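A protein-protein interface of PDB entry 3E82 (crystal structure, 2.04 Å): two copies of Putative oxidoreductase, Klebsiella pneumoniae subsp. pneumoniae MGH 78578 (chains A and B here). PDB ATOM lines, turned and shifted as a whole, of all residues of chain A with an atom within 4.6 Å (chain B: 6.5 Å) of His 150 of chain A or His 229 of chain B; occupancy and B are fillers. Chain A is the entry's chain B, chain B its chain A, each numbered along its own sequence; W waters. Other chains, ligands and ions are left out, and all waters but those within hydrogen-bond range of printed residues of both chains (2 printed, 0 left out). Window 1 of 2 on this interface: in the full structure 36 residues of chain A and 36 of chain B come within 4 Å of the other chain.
The backbone carbonyl oxygen (O) of Leu 205 of chain B is in hydrogen-bond range of the side-chain amino group (NZ) of Lys 149 of chain A, at 2.9 Å. The indole nitrogen (NE1) of Trp 214 of chain B is in hydrogen-bond range of a ring nitrogen (ND1) of His 150 of chain A (3.1 Å).
The backbone carbonyl oxygen (O) of Ser 153 of chain B lies within hydrogen-bond range of the backbone NH (N) of His 229 of chain B. ND1 of His 229 of chain B lies within hydrogen-bond range of OD1 of Asp 156 of chain B, 3.4 Å away. The indole nitrogen (NE1) of Trp 214 of chain B is in hydrogen-bond range of a ring nitrogen (NE2) of His 229 of chain B, 3.4 Å away. The backbone NH of Lys 149 of chain A lies within hydrogen-bond range of the backbone carbonyl oxygen of His 244 of chain A (2.9 Å). The backbone carbonyl oxygen of His 150 of chain A is in hydrogen-bond range of the backbone NH of His 244 of chain A (2.7 Å). The backbone carbonyl oxygen of Lys 225 of chain A lies within hydrogen-bond range of the backbone NH of Phe 151 of chain A (3.0 Å).
Among the printed residues, pairs that only touch across the chains: His 244 of chain A with Leu 233 of chain B, Lys 225 of chain A with Trp 214 of chain B, His 150 of chain A with His 229 of chain B, Ile 227 of chain A with His 216 of chain B, Lys 149 of chain A with Leu 233 of chain B and His 244 of chain A with Val 234 of chain B.
Of chain B, only Trp 214 (3.1 Å) and His 229 (3.6 Å) come within 4 Å of His 150 of chain A. His 229 of chain B touches just one residue of chain A: His 150 (3.6 Å). Of the printed residues of chain A, Leu 205 of chain B touches Lys 149. Of the printed residues of chain A, Trp 214 of chain B touches His 150 and Lys 225. Of the printed residues of chain B, Lys 149 of chain A touches Leu 205 (2.9 Å) and Leu 233 (3.7 Å). Of the printed residues of chain A, His 216 of chain B touches Ile 227 (3.6 Å). Printed residues of chain B within 4 Å of Lys 225 of chain A: Trp 214 (3.5 Å). The nearest printed residue of chain A that does not touch His 229 of chain B is Ile 227 of chain A (5.0 Å).
Of the 10 printed residues of chain A, 5 touch a printed residue of chain B. Printed residues of chain A that touch a printed residue of chain B: Lys 149, His 150, Lys 225, Ile 227 and His 244. Of the 19 printed residues of chain B, 6 touch a printed residue of chain A.
Positions printed for both chains: 152 and 227. Of the 8 pairs that touch across the chains among the printed residues, none has its exchanged pair printed and touching as well.
Water W1 bridges OE2 of Glu 152 of chain B (2.6 Å) and OE2 of Glu 152 of chain A (2.8 Å). Water W2 lies within hydrogen-bond range of ND1 of His 150 of chain A and NE2 of His 229 of chain B.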
ATOM      1  N   VAL A 148      -0.898  -3.473   6.824  1.00  0.00           N
ATOM      2  CA  VAL A 148      -1.887  -3.179   5.782  1.00  0.00           C
ATOM      3  C   VAL A 148      -2.508  -1.798   6.009  1.00  0.00           C
ATOM      4  O   VAL A 148      -2.887  -1.456   7.130  1.00  0.00           O
ATOM      5  CB  VAL A 148      -3.010  -4.246   5.750  1.00  0.00           C
ATOM      6  CG1 VAL A 148      -4.124  -3.811   4.797  1.00  0.00           C
ATOM      7  CG2 VAL A 148      -2.436  -5.582   5.301  1.00  0.00           C
ATOM      8  N   LYS A 149      -2.613  -1.011   4.939  1.00  0.00           N
ATOM      9  CA  LYS A 149      -3.162   0.333   5.034  1.00  0.00           C
ATOM     10  C   LYS A 149      -4.360   0.561   4.113  1.00  0.00           C
ATOM     11  O   LYS A 149      -5.224   1.396   4.402  1.00  0.00           O
ATOM     12  CB  LYS A 149      -2.059   1.368   4.738  1.00  0.00           C
ATOM     13  CG  LYS A 149      -0.971   1.414   5.819  1.00  0.00           C
ATOM     14  CD  LYS A 149      -1.603   1.724   7.168  1.00  0.00           C
ATOM     15  CE  LYS A 149      -0.725   1.303   8.340  1.00  0.00           C
ATOM     16  NZ  LYS A 149       0.508   2.110   8.440  1.00  0.00           N
ATOM     17  N   HIS A 150      -4.408  -0.199   3.021  1.00  0.00           N
ATOM     18  CA  HIS A 150      -5.472  -0.088   2.028  1.00  0.00           C
ATOM     19  C   HIS A 150      -5.798  -1.474   1.458  1.00  0.00           C
ATOM     20  O   HIS A 150      -4.994  -2.073   0.738  1.00  0.00           O
ATOM     21  CB  HIS A 150      -5.022   0.875   0.911  1.00  0.00           C
ATOM     22  CG  HIS A 150      -6.005   1.030  -0.213  1.00  0.00           C
ATOM     23  ND1 HIS A 150      -6.478   2.259  -0.620  1.00  0.00           N
ATOM     24  CD2 HIS A 150      -6.573   0.119  -1.040  1.00  0.00           C
ATOM     25  CE1 HIS A 150      -7.293   2.100  -1.649  1.00  0.00           C
ATOM     26  NE2 HIS A 150      -7.368   0.809  -1.923  1.00  0.00           N
ATOM     27  N   PHE A 151      -6.986  -1.972   1.798  1.00  0.00           N
ATOM     28  CA  PHE A 151      -7.467  -3.282   1.356  1.00  0.00           C
ATOM     29  C   PHE A 151      -8.664  -3.045   0.435  1.00  0.00           C
ATOM     30  O   PHE A 151      -9.677  -2.472   0.849  1.00  0.00           O
ATOM     31  CB  PHE A 151      -7.888  -4.106   2.576  1.00  0.00           C
ATOM     32  CG  PHE A 151      -8.403  -5.489   2.248  1.00  0.00           C
ATOM     33  CD1 PHE A 151      -7.540  -6.583   2.219  1.00  0.00           C
ATOM     34  CD2 PHE A 151      -9.758  -5.703   2.029  1.00  0.00           C
ATOM     35  CE1 PHE A 151      -8.026  -7.865   1.983  1.00  0.00           C
ATOM     36  CE2 PHE A 151     -10.252  -6.984   1.792  1.00  0.00           C
ATOM     37  CZ  PHE A 151      -9.389  -8.062   1.771  1.00  0.00           C
ATOM     38  N   GLU A 152      -8.542  -3.474  -0.817  1.00  0.00           N
ATOM     39  CA  GLU A 152      -9.604  -3.275  -1.794  1.00  0.00           C
ATOM     40  C   GLU A 152     -10.058  -4.600  -2.402  1.00  0.00           C
ATOM     41  O   GLU A 152      -9.242  -5.379  -2.913  1.00  0.00           O
ATOM     42  CB  GLU A 152      -9.119  -2.324  -2.893  1.00  0.00           C
ATOM     43  CG  GLU A 152     -10.224  -1.809  -3.781  1.00  0.00           C
ATOM     44  CD  GLU A 152      -9.784  -0.644  -4.631  1.00  0.00           C
ATOM     45  OE1 GLU A 152      -8.817   0.048  -4.240  1.00  0.00           O
ATOM     46  OE2 GLU A 152     -10.422  -0.413  -5.680  1.00  0.00           O
ATOM     47  N   LYS A 225      -7.856   1.504   5.762  1.00  0.00           N
ATOM     48  CA  LYS A 225      -9.108   1.607   5.024  1.00  0.00           C
ATOM     49  C   LYS A 225      -9.433   0.349   4.232  1.00  0.00           C
ATOM     50  O   LYS A 225      -8.543  -0.337   3.720  1.00  0.00           O
ATOM     51  CB  LYS A 225      -9.040   2.794   4.050  1.00  0.00           C
ATOM     52  CG  LYS A 225      -8.736   4.146   4.698  1.00  0.00           C
ATOM     53  CD  LYS A 225      -9.891   4.619   5.583  1.00  0.00           C
ATOM     54  CE  LYS A 225      -9.594   5.993   6.191  1.00  0.00           C
ATOM     55  NZ  LYS A 225     -10.695   6.510   7.045  1.00  0.00           N
ATOM     56  N   ILE A 227     -12.001  -0.917   1.107  1.00  0.00           N
ATOM     57  CA  ILE A 227     -12.895  -0.512   0.037  1.00  0.00           C
ATOM     58  C   ILE A 227     -13.489  -1.750  -0.626  1.00  0.00           C
ATOM     59  O   ILE A 227     -12.756  -2.628  -1.094  1.00  0.00           O
ATOM     60  CB  ILE A 227     -12.152   0.317  -1.033  1.00  0.00           C
ATOM     61  CG1 ILE A 227     -11.700   1.652  -0.437  1.00  0.00           C
ATOM     62  CG2 ILE A 227     -13.068   0.565  -2.223  1.00  0.00           C
ATOM     63  CD1 ILE A 227     -10.908   2.517  -1.417  1.00  0.00           C
ATOM     64  N   THR A 242      -6.807  -5.841  -4.267  1.00  0.00           N
ATOM     65  CA  THR A 242      -5.696  -4.902  -4.368  1.00  0.00           C
ATOM     66  C   THR A 242      -5.420  -4.516  -2.917  1.00  0.00           C
ATOM     67  O   THR A 242      -6.288  -3.959  -2.250  1.00  0.00           O
ATOM     68  CB  THR A 242      -6.070  -3.630  -5.166  1.00  0.00           C
ATOM     69  OG1 THR A 242      -6.347  -3.980  -6.528  1.00  0.00           O
ATOM     70  CG2 THR A 242      -4.922  -2.628  -5.127  1.00  0.00           C
ATOM     71  N   VAL A 243      -4.227  -4.832  -2.425  1.00  0.00           N
ATOM     72  CA  VAL A 243      -3.879  -4.524  -1.039  1.00  0.00           C
ATOM     73  C   VAL A 243      -2.532  -3.834  -0.939  1.00  0.00           C
ATOM     74  O   VAL A 243      -1.531  -4.340  -1.447  1.00  0.00           O
ATOM     75  CB  VAL A 243      -3.842  -5.806  -0.177  1.00  0.00           C
ATOM     76  CG1 VAL A 243      -3.601  -5.453   1.292  1.00  0.00           C
ATOM     77  CG2 VAL A 243      -5.147  -6.568  -0.336  1.00  0.00           C
ATOM     78  N   HIS A 244      -2.514  -2.676  -0.281  1.00  0.00           N
ATOM     79  CA  HIS A 244      -1.287  -1.908  -0.113  1.00  0.00           C
ATOM     80  C   HIS A 244      -0.908  -1.815   1.352  1.00  0.00           C
ATOM     81  O   HIS A 244      -1.747  -1.512   2.207  1.00  0.00           O
ATOM     82  CB  HIS A 244      -1.457  -0.484  -0.661  1.00  0.00           C
ATOM     83  CG  HIS A 244      -2.005  -0.430  -2.053  1.00  0.00           C
ATOM     84  ND1 HIS A 244      -1.354  -0.986  -3.134  1.00  0.00           N
ATOM     85  CD2 HIS A 244      -3.145   0.113  -2.537  1.00  0.00           C
ATOM     86  CE1 HIS A 244      -2.073  -0.790  -4.224  1.00  0.00           C
ATOM     87  NE2 HIS A 244      -3.165  -0.126  -3.890  1.00  0.00           N
ATOM     88  N   GLU B 152     -12.391   7.037 -12.776  1.00  0.00           N
ATOM     89  CA  GLU B 152     -11.457   6.950 -11.655  1.00  0.00           C
ATOM     90  C   GLU B 152     -10.093   7.518 -12.033  1.00  0.00           C
ATOM     91  O   GLU B 152      -9.532   7.161 -13.071  1.00  0.00           O
ATOM     92  CB  GLU B 152     -11.320   5.492 -11.200  1.00  0.00           C
ATOM     93  CG  GLU B 152     -10.629   5.324  -9.863  1.00  0.00           C
ATOM     94  CD  GLU B 152     -10.819   3.934  -9.285  1.00  0.00           C
ATOM     95  OE1 GLU B 152     -11.773   3.237  -9.704  1.00  0.00           O
ATOM     96  OE2 GLU B 152     -10.022   3.547  -8.402  1.00  0.00           O
ATOM     97  N   SER B 153      -9.570   8.389 -11.167  1.00  0.00           N
ATOM     98  CA  SER B 153      -8.303   9.085 -11.381  1.00  0.00           C
ATOM     99  C   SER B 153      -7.423   9.000 -10.137  1.00  0.00           C
ATOM    100  O   SER B 153      -7.827   9.431  -9.051  1.00  0.00           O
ATOM    101  CB  SER B 153      -8.604  10.550 -11.719  1.00  0.00           C
ATOM    102  OG  SER B 153      -7.429  11.331 -11.809  1.00  0.00           O
ATOM    103  N   HIS B 154      -6.223   8.449 -10.306  1.00  0.00           N
ATOM    104  CA  HIS B 154      -5.277   8.259  -9.205  1.00  0.00           C
ATOM    105  C   HIS B 154      -3.954   8.997  -9.319  1.00  0.00           C
ATOM    106  O   HIS B 154      -3.391   9.123 -10.406  1.00  0.00           O
ATOM    107  CB  HIS B 154      -4.888   6.781  -9.069  1.00  0.00           C
ATOM    108  CG  HIS B 154      -5.938   5.906  -8.462  1.00  0.00           C
ATOM    109  ND1 HIS B 154      -5.699   5.128  -7.349  1.00  0.00           N
ATOM    110  CD2 HIS B 154      -7.215   5.652  -8.834  1.00  0.00           C
ATOM    111  CE1 HIS B 154      -6.783   4.431  -7.062  1.00  0.00           C
ATOM    112  NE2 HIS B 154      -7.718   4.731  -7.948  1.00  0.00           N
ATOM    113  N   PHE B 155      -3.455   9.452  -8.175  1.00  0.00           N
ATOM    114  CA  PHE B 155      -2.129  10.060  -8.079  1.00  0.00           C
ATOM    115  C   PHE B 155      -1.518   9.267  -6.916  1.00  0.00           C
ATOM    116  O   PHE B 155      -1.645   9.640  -5.750  1.00  0.00           O
ATOM    117  CB  PHE B 155      -2.196  11.560  -7.761  1.00  0.00           C
ATOM    118  CG  PHE B 155      -2.267  12.443  -8.995  1.00  0.00           C
ATOM    119  CD1 PHE B 155      -1.631  12.066 -10.180  1.00  0.00           C
ATOM    120  CD2 PHE B 155      -2.925  13.673  -8.957  1.00  0.00           C
ATOM    121  CE1 PHE B 155      -1.648  12.893 -11.302  1.00  0.00           C
ATOM    122  CE2 PHE B 155      -2.947  14.514 -10.082  1.00  0.00           C
ATOM    123  CZ  PHE B 155      -2.307  14.123 -11.253  1.00  0.00           C
ATOM    124  N   ASP B 156      -0.898   8.137  -7.245  1.00  0.00           N
ATOM    125  CA  ASP B 156      -0.310   7.267  -6.235  1.00  0.00           C
ATOM    126  C   ASP B 156       1.181   7.057  -6.409  1.00  0.00           C
ATOM    127  O   ASP B 156       1.713   7.110  -7.519  1.00  0.00           O
ATOM    128  CB  ASP B 156      -0.964   5.876  -6.256  1.00  0.00           C
ATOM    129  CG  ASP B 156      -2.455   5.903  -5.948  1.00  0.00           C
ATOM    130  OD1 ASP B 156      -2.918   6.814  -5.223  1.00  0.00           O
ATOM    131  OD2 ASP B 156      -3.160   4.984  -6.421  1.00  0.00           O
ATOM    132  N   TRP B 177      -3.940  15.788  -0.038  1.00  0.00           N
ATOM    133  CA  TRP B 177      -5.167  16.237  -0.694  1.00  0.00           C
ATOM    134  C   TRP B 177      -5.010  17.659  -1.247  1.00  0.00           C
ATOM    135  O   TRP B 177      -5.309  17.927  -2.411  1.00  0.00           O
ATOM    136  CB  TRP B 177      -6.352  16.185   0.275  1.00  0.00           C
ATOM    137  CG  TRP B 177      -7.649  16.637  -0.338  1.00  0.00           C
ATOM    138  CD1 TRP B 177      -8.481  17.625   0.124  1.00  0.00           C
ATOM    139  CD2 TRP B 177      -8.256  16.131  -1.534  1.00  0.00           C
ATOM    140  NE1 TRP B 177      -9.562  17.763  -0.709  1.00  0.00           N
ATOM    141  CE2 TRP B 177      -9.452  16.860  -1.736  1.00  0.00           C
ATOM    142  CE3 TRP B 177      -7.906  15.132  -2.456  1.00  0.00           C
ATOM    143  CZ2 TRP B 177     -10.303  16.622  -2.827  1.00  0.00           C
ATOM    144  CZ3 TRP B 177      -8.753  14.894  -3.542  1.00  0.00           C
ATOM    145  CH2 TRP B 177      -9.936  15.639  -3.715  1.00  0.00           C
ATOM    146  N   LEU B 184      -6.450  16.627  -9.876  1.00  0.00           N
ATOM    147  CA  LEU B 184      -7.526  15.648 -10.035  1.00  0.00           C
ATOM    148  C   LEU B 184      -8.897  16.305 -10.214  1.00  0.00           C
ATOM    149  O   LEU B 184      -9.680  15.917 -11.081  1.00  0.00           O
ATOM    150  CB  LEU B 184      -7.566  14.736  -8.807  1.00  0.00           C
ATOM    151  CG  LEU B 184      -6.276  13.965  -8.520  1.00  0.00           C
ATOM    152  CD1 LEU B 184      -6.391  13.209  -7.192  1.00  0.00           C
ATOM    153  CD2 LEU B 184      -6.016  13.002  -9.666  1.00  0.00           C
ATOM    154  N   LEU B 205      -2.146   7.765   7.189  1.00  0.00           N
ATOM    155  CA  LEU B 205      -1.906   6.357   7.479  1.00  0.00           C
ATOM    156  C   LEU B 205      -0.469   5.887   7.670  1.00  0.00           C
ATOM    157  O   LEU B 205      -0.242   4.865   8.321  1.00  0.00           O
ATOM    158  CB  LEU B 205      -2.582   5.510   6.398  1.00  0.00           C
ATOM    159  CG  LEU B 205      -4.093   5.752   6.246  1.00  0.00           C
ATOM    160  CD1 LEU B 205      -4.624   5.029   5.013  1.00  0.00           C
ATOM    161  CD2 LEU B 205      -4.815   5.271   7.495  1.00  0.00           C
ATOM    162  N   TRP B 214      -3.446   9.931   2.387  1.00  0.00           N
ATOM    163  CA  TRP B 214      -4.441   9.066   1.772  1.00  0.00           C
ATOM    164  C   TRP B 214      -5.726   9.893   1.652  1.00  0.00           C
ATOM    165  O   TRP B 214      -6.255  10.388   2.659  1.00  0.00           O
ATOM    166  CB  TRP B 214      -4.701   7.844   2.654  1.00  0.00           C
ATOM    167  CG  TRP B 214      -5.534   6.773   2.011  1.00  0.00           C
ATOM    168  CD1 TRP B 214      -5.079   5.690   1.313  1.00  0.00           C
ATOM    169  CD2 TRP B 214      -6.963   6.662   2.033  1.00  0.00           C
ATOM    170  NE1 TRP B 214      -6.134   4.911   0.905  1.00  0.00           N
ATOM    171  CE2 TRP B 214      -7.301   5.483   1.334  1.00  0.00           C
ATOM    172  CE3 TRP B 214      -7.991   7.442   2.580  1.00  0.00           C
ATOM    173  CZ2 TRP B 214      -8.627   5.064   1.164  1.00  0.00           C
ATOM    174  CZ3 TRP B 214      -9.306   7.026   2.414  1.00  0.00           C
ATOM    175  CH2 TRP B 214      -9.610   5.849   1.712  1.00  0.00           C
ATOM    176  N   ALA B 215      -6.210  10.060   0.425  1.00  0.00           N
ATOM    177  CA  ALA B 215      -7.430  10.813   0.180  1.00  0.00           C
ATOM    178  C   ALA B 215      -8.275  10.068  -0.851  1.00  0.00           C
ATOM    179  O   ALA B 215      -7.806   9.735  -1.944  1.00  0.00           O
ATOM    180  CB  ALA B 215      -7.101  12.225  -0.308  1.00  0.00           C
ATOM    181  N   HIS B 216      -9.522   9.797  -0.486  1.00  0.00           N
ATOM    182  CA  HIS B 216     -10.441   9.078  -1.358  1.00  0.00           C
ATOM    183  C   HIS B 216     -11.704   9.931  -1.456  1.00  0.00           C
ATOM    184  O   HIS B 216     -12.507   9.995  -0.524  1.00  0.00           O
ATOM    185  CB  HIS B 216     -10.737   7.700  -0.755  1.00  0.00           C
ATOM    186  CG  HIS B 216     -11.403   6.756  -1.705  1.00  0.00           C
ATOM    187  ND1 HIS B 216     -12.712   6.354  -1.560  1.00  0.00           N
ATOM    188  CD2 HIS B 216     -10.949   6.156  -2.831  1.00  0.00           C
ATOM    189  CE1 HIS B 216     -13.033   5.550  -2.556  1.00  0.00           C
ATOM    190  NE2 HIS B 216     -11.981   5.414  -3.343  1.00  0.00           N
ATOM    191  N   VAL B 217     -11.866  10.584  -2.603  1.00  0.00           N
ATOM    192  CA  VAL B 217     -12.974  11.506  -2.822  1.00  0.00           C
ATOM    193  C   VAL B 217     -13.893  11.117  -3.969  1.00  0.00           C
ATOM    194  O   VAL B 217     -13.444  10.841  -5.079  1.00  0.00           O
ATOM    195  CB  VAL B 217     -12.403  12.916  -3.062  1.00  0.00           C
ATOM    196  CG1 VAL B 217     -13.514  13.915  -3.452  1.00  0.00           C
ATOM    197  CG2 VAL B 217     -11.688  13.371  -1.811  1.00  0.00           C
ATOM    198  N   ILE B 227     -14.300   9.093  -9.078  1.00  0.00           N
ATOM    199  CA  ILE B 227     -13.477   8.770  -7.925  1.00  0.00           C
ATOM    200  C   ILE B 227     -12.088   9.387  -8.079  1.00  0.00           C
ATOM    201  O   ILE B 227     -11.373   9.107  -9.055  1.00  0.00           O
ATOM    202  CB  ILE B 227     -13.323   7.242  -7.741  1.00  0.00           C
ATOM    203  CG1 ILE B 227     -14.671   6.629  -7.349  1.00  0.00           C
ATOM    204  CG2 ILE B 227     -12.280   6.945  -6.669  1.00  0.00           C
ATOM    205  CD1 ILE B 227     -14.601   5.151  -7.024  1.00  0.00           C
ATOM    206  N   LEU B 228     -11.731  10.249  -7.129  1.00  0.00           N
ATOM    207  CA  LEU B 228     -10.427  10.904  -7.120  1.00  0.00           C
ATOM    208  C   LEU B 228      -9.686  10.295  -5.943  1.00  0.00           C
ATOM    209  O   LEU B 228     -10.180  10.311  -4.815  1.00  0.00           O
ATOM    210  CB  LEU B 228     -10.577  12.412  -6.927  1.00  0.00           C
ATOM    211  CG  LEU B 228     -11.506  13.123  -7.920  1.00  0.00           C
ATOM    212  CD1 LEU B 228     -11.449  14.624  -7.652  1.00  0.00           C
ATOM    213  CD2 LEU B 228     -11.079  12.833  -9.368  1.00  0.00           C
ATOM    214  N   HIS B 229      -8.500   9.764  -6.207  1.00  0.00           N
ATOM    215  CA  HIS B 229      -7.732   9.094  -5.172  1.00  0.00           C
ATOM    216  C   HIS B 229      -6.239   9.376  -5.237  1.00  0.00           C
ATOM    217  O   HIS B 229      -5.656   9.422  -6.313  1.00  0.00           O
ATOM    218  CB  HIS B 229      -7.955   7.580  -5.301  1.00  0.00           C
ATOM    219  CG  HIS B 229      -7.421   6.784  -4.151  1.00  0.00           C
ATOM    220  ND1 HIS B 229      -6.094   6.433  -4.034  1.00  0.00           N
ATOM    221  CD2 HIS B 229      -8.039   6.291  -3.054  1.00  0.00           C
ATOM    222  CE1 HIS B 229      -5.916   5.757  -2.913  1.00  0.00           C
ATOM    223  NE2 HIS B 229      -7.082   5.657  -2.299  1.00  0.00           N
ATOM    224  N   CYS B 230      -5.628   9.569  -4.080  1.00  0.00           N
ATOM    225  CA  CYS B 230      -4.191   9.758  -4.019  1.00  0.00           C
ATOM    226  C   CYS B 230      -3.671   9.192  -2.709  1.00  0.00           C
ATOM    227  O   CYS B 230      -4.320   9.298  -1.667  1.00  0.00           O
ATOM    228  CB  CYS B 230      -3.787  11.230  -4.208  1.00  0.00           C
ATOM    229  SG  CYS B 230      -4.622  12.452  -3.199  1.00  0.00           S
ATOM    230  N   SER B 231      -2.514   8.548  -2.787  1.00  0.00           N
ATOM    231  CA  SER B 231      -1.897   7.934  -1.628  1.00  0.00           C
ATOM    232  C   SER B 231      -0.384   7.913  -1.738  1.00  0.00           C
ATOM    233  O   SER B 231       0.166   7.807  -2.838  1.00  0.00           O
ATOM    234  CB  SER B 231      -2.400   6.499  -1.471  1.00  0.00           C
ATOM    235  OG  SER B 231      -1.667   5.808  -0.471  1.00  0.00           O
ATOM    236  N   LEU B 233       1.265   5.588  -0.132  1.00  0.00           N
ATOM    237  CA  LEU B 233       1.620   4.192   0.134  1.00  0.00           C
ATOM    238  C   LEU B 233       1.093   3.201  -0.902  1.00  0.00           C
ATOM    239  O   LEU B 233       0.229   2.367  -0.602  1.00  0.00           O
ATOM    240  CB  LEU B 233       1.132   3.767   1.523  1.00  0.00           C
ATOM    241  CG  LEU B 233       1.924   4.239   2.737  1.00  0.00           C
ATOM    242  CD1 LEU B 233       1.221   3.795   4.019  1.00  0.00           C
ATOM    243  CD2 LEU B 233       3.335   3.673   2.671  1.00  0.00           C
ATOM    244  N   VAL B 234       1.623   3.287  -2.118  1.00  0.00           N
ATOM    245  CA  VAL B 234       1.210   2.395  -3.198  1.00  0.00           C
ATOM    246  C   VAL B 234       2.458   1.886  -3.932  1.00  0.00           C
ATOM    247  O   VAL B 234       2.964   2.542  -4.842  1.00  0.00           O
ATOM    248  CB  VAL B 234       0.288   3.126  -4.209  1.00  0.00           C
ATOM    249  CG1 VAL B 234      -0.045   2.212  -5.373  1.00  0.00           C
ATOM    250  CG2 VAL B 234      -0.985   3.571  -3.522  1.00  0.00           C
HETATM  251  O   HOH W   1      -9.537   1.045  -7.841  1.00  0.00           O
HETATM  252  O   HOH W   2      -4.248   3.684  -1.889  1.00  0.00           O
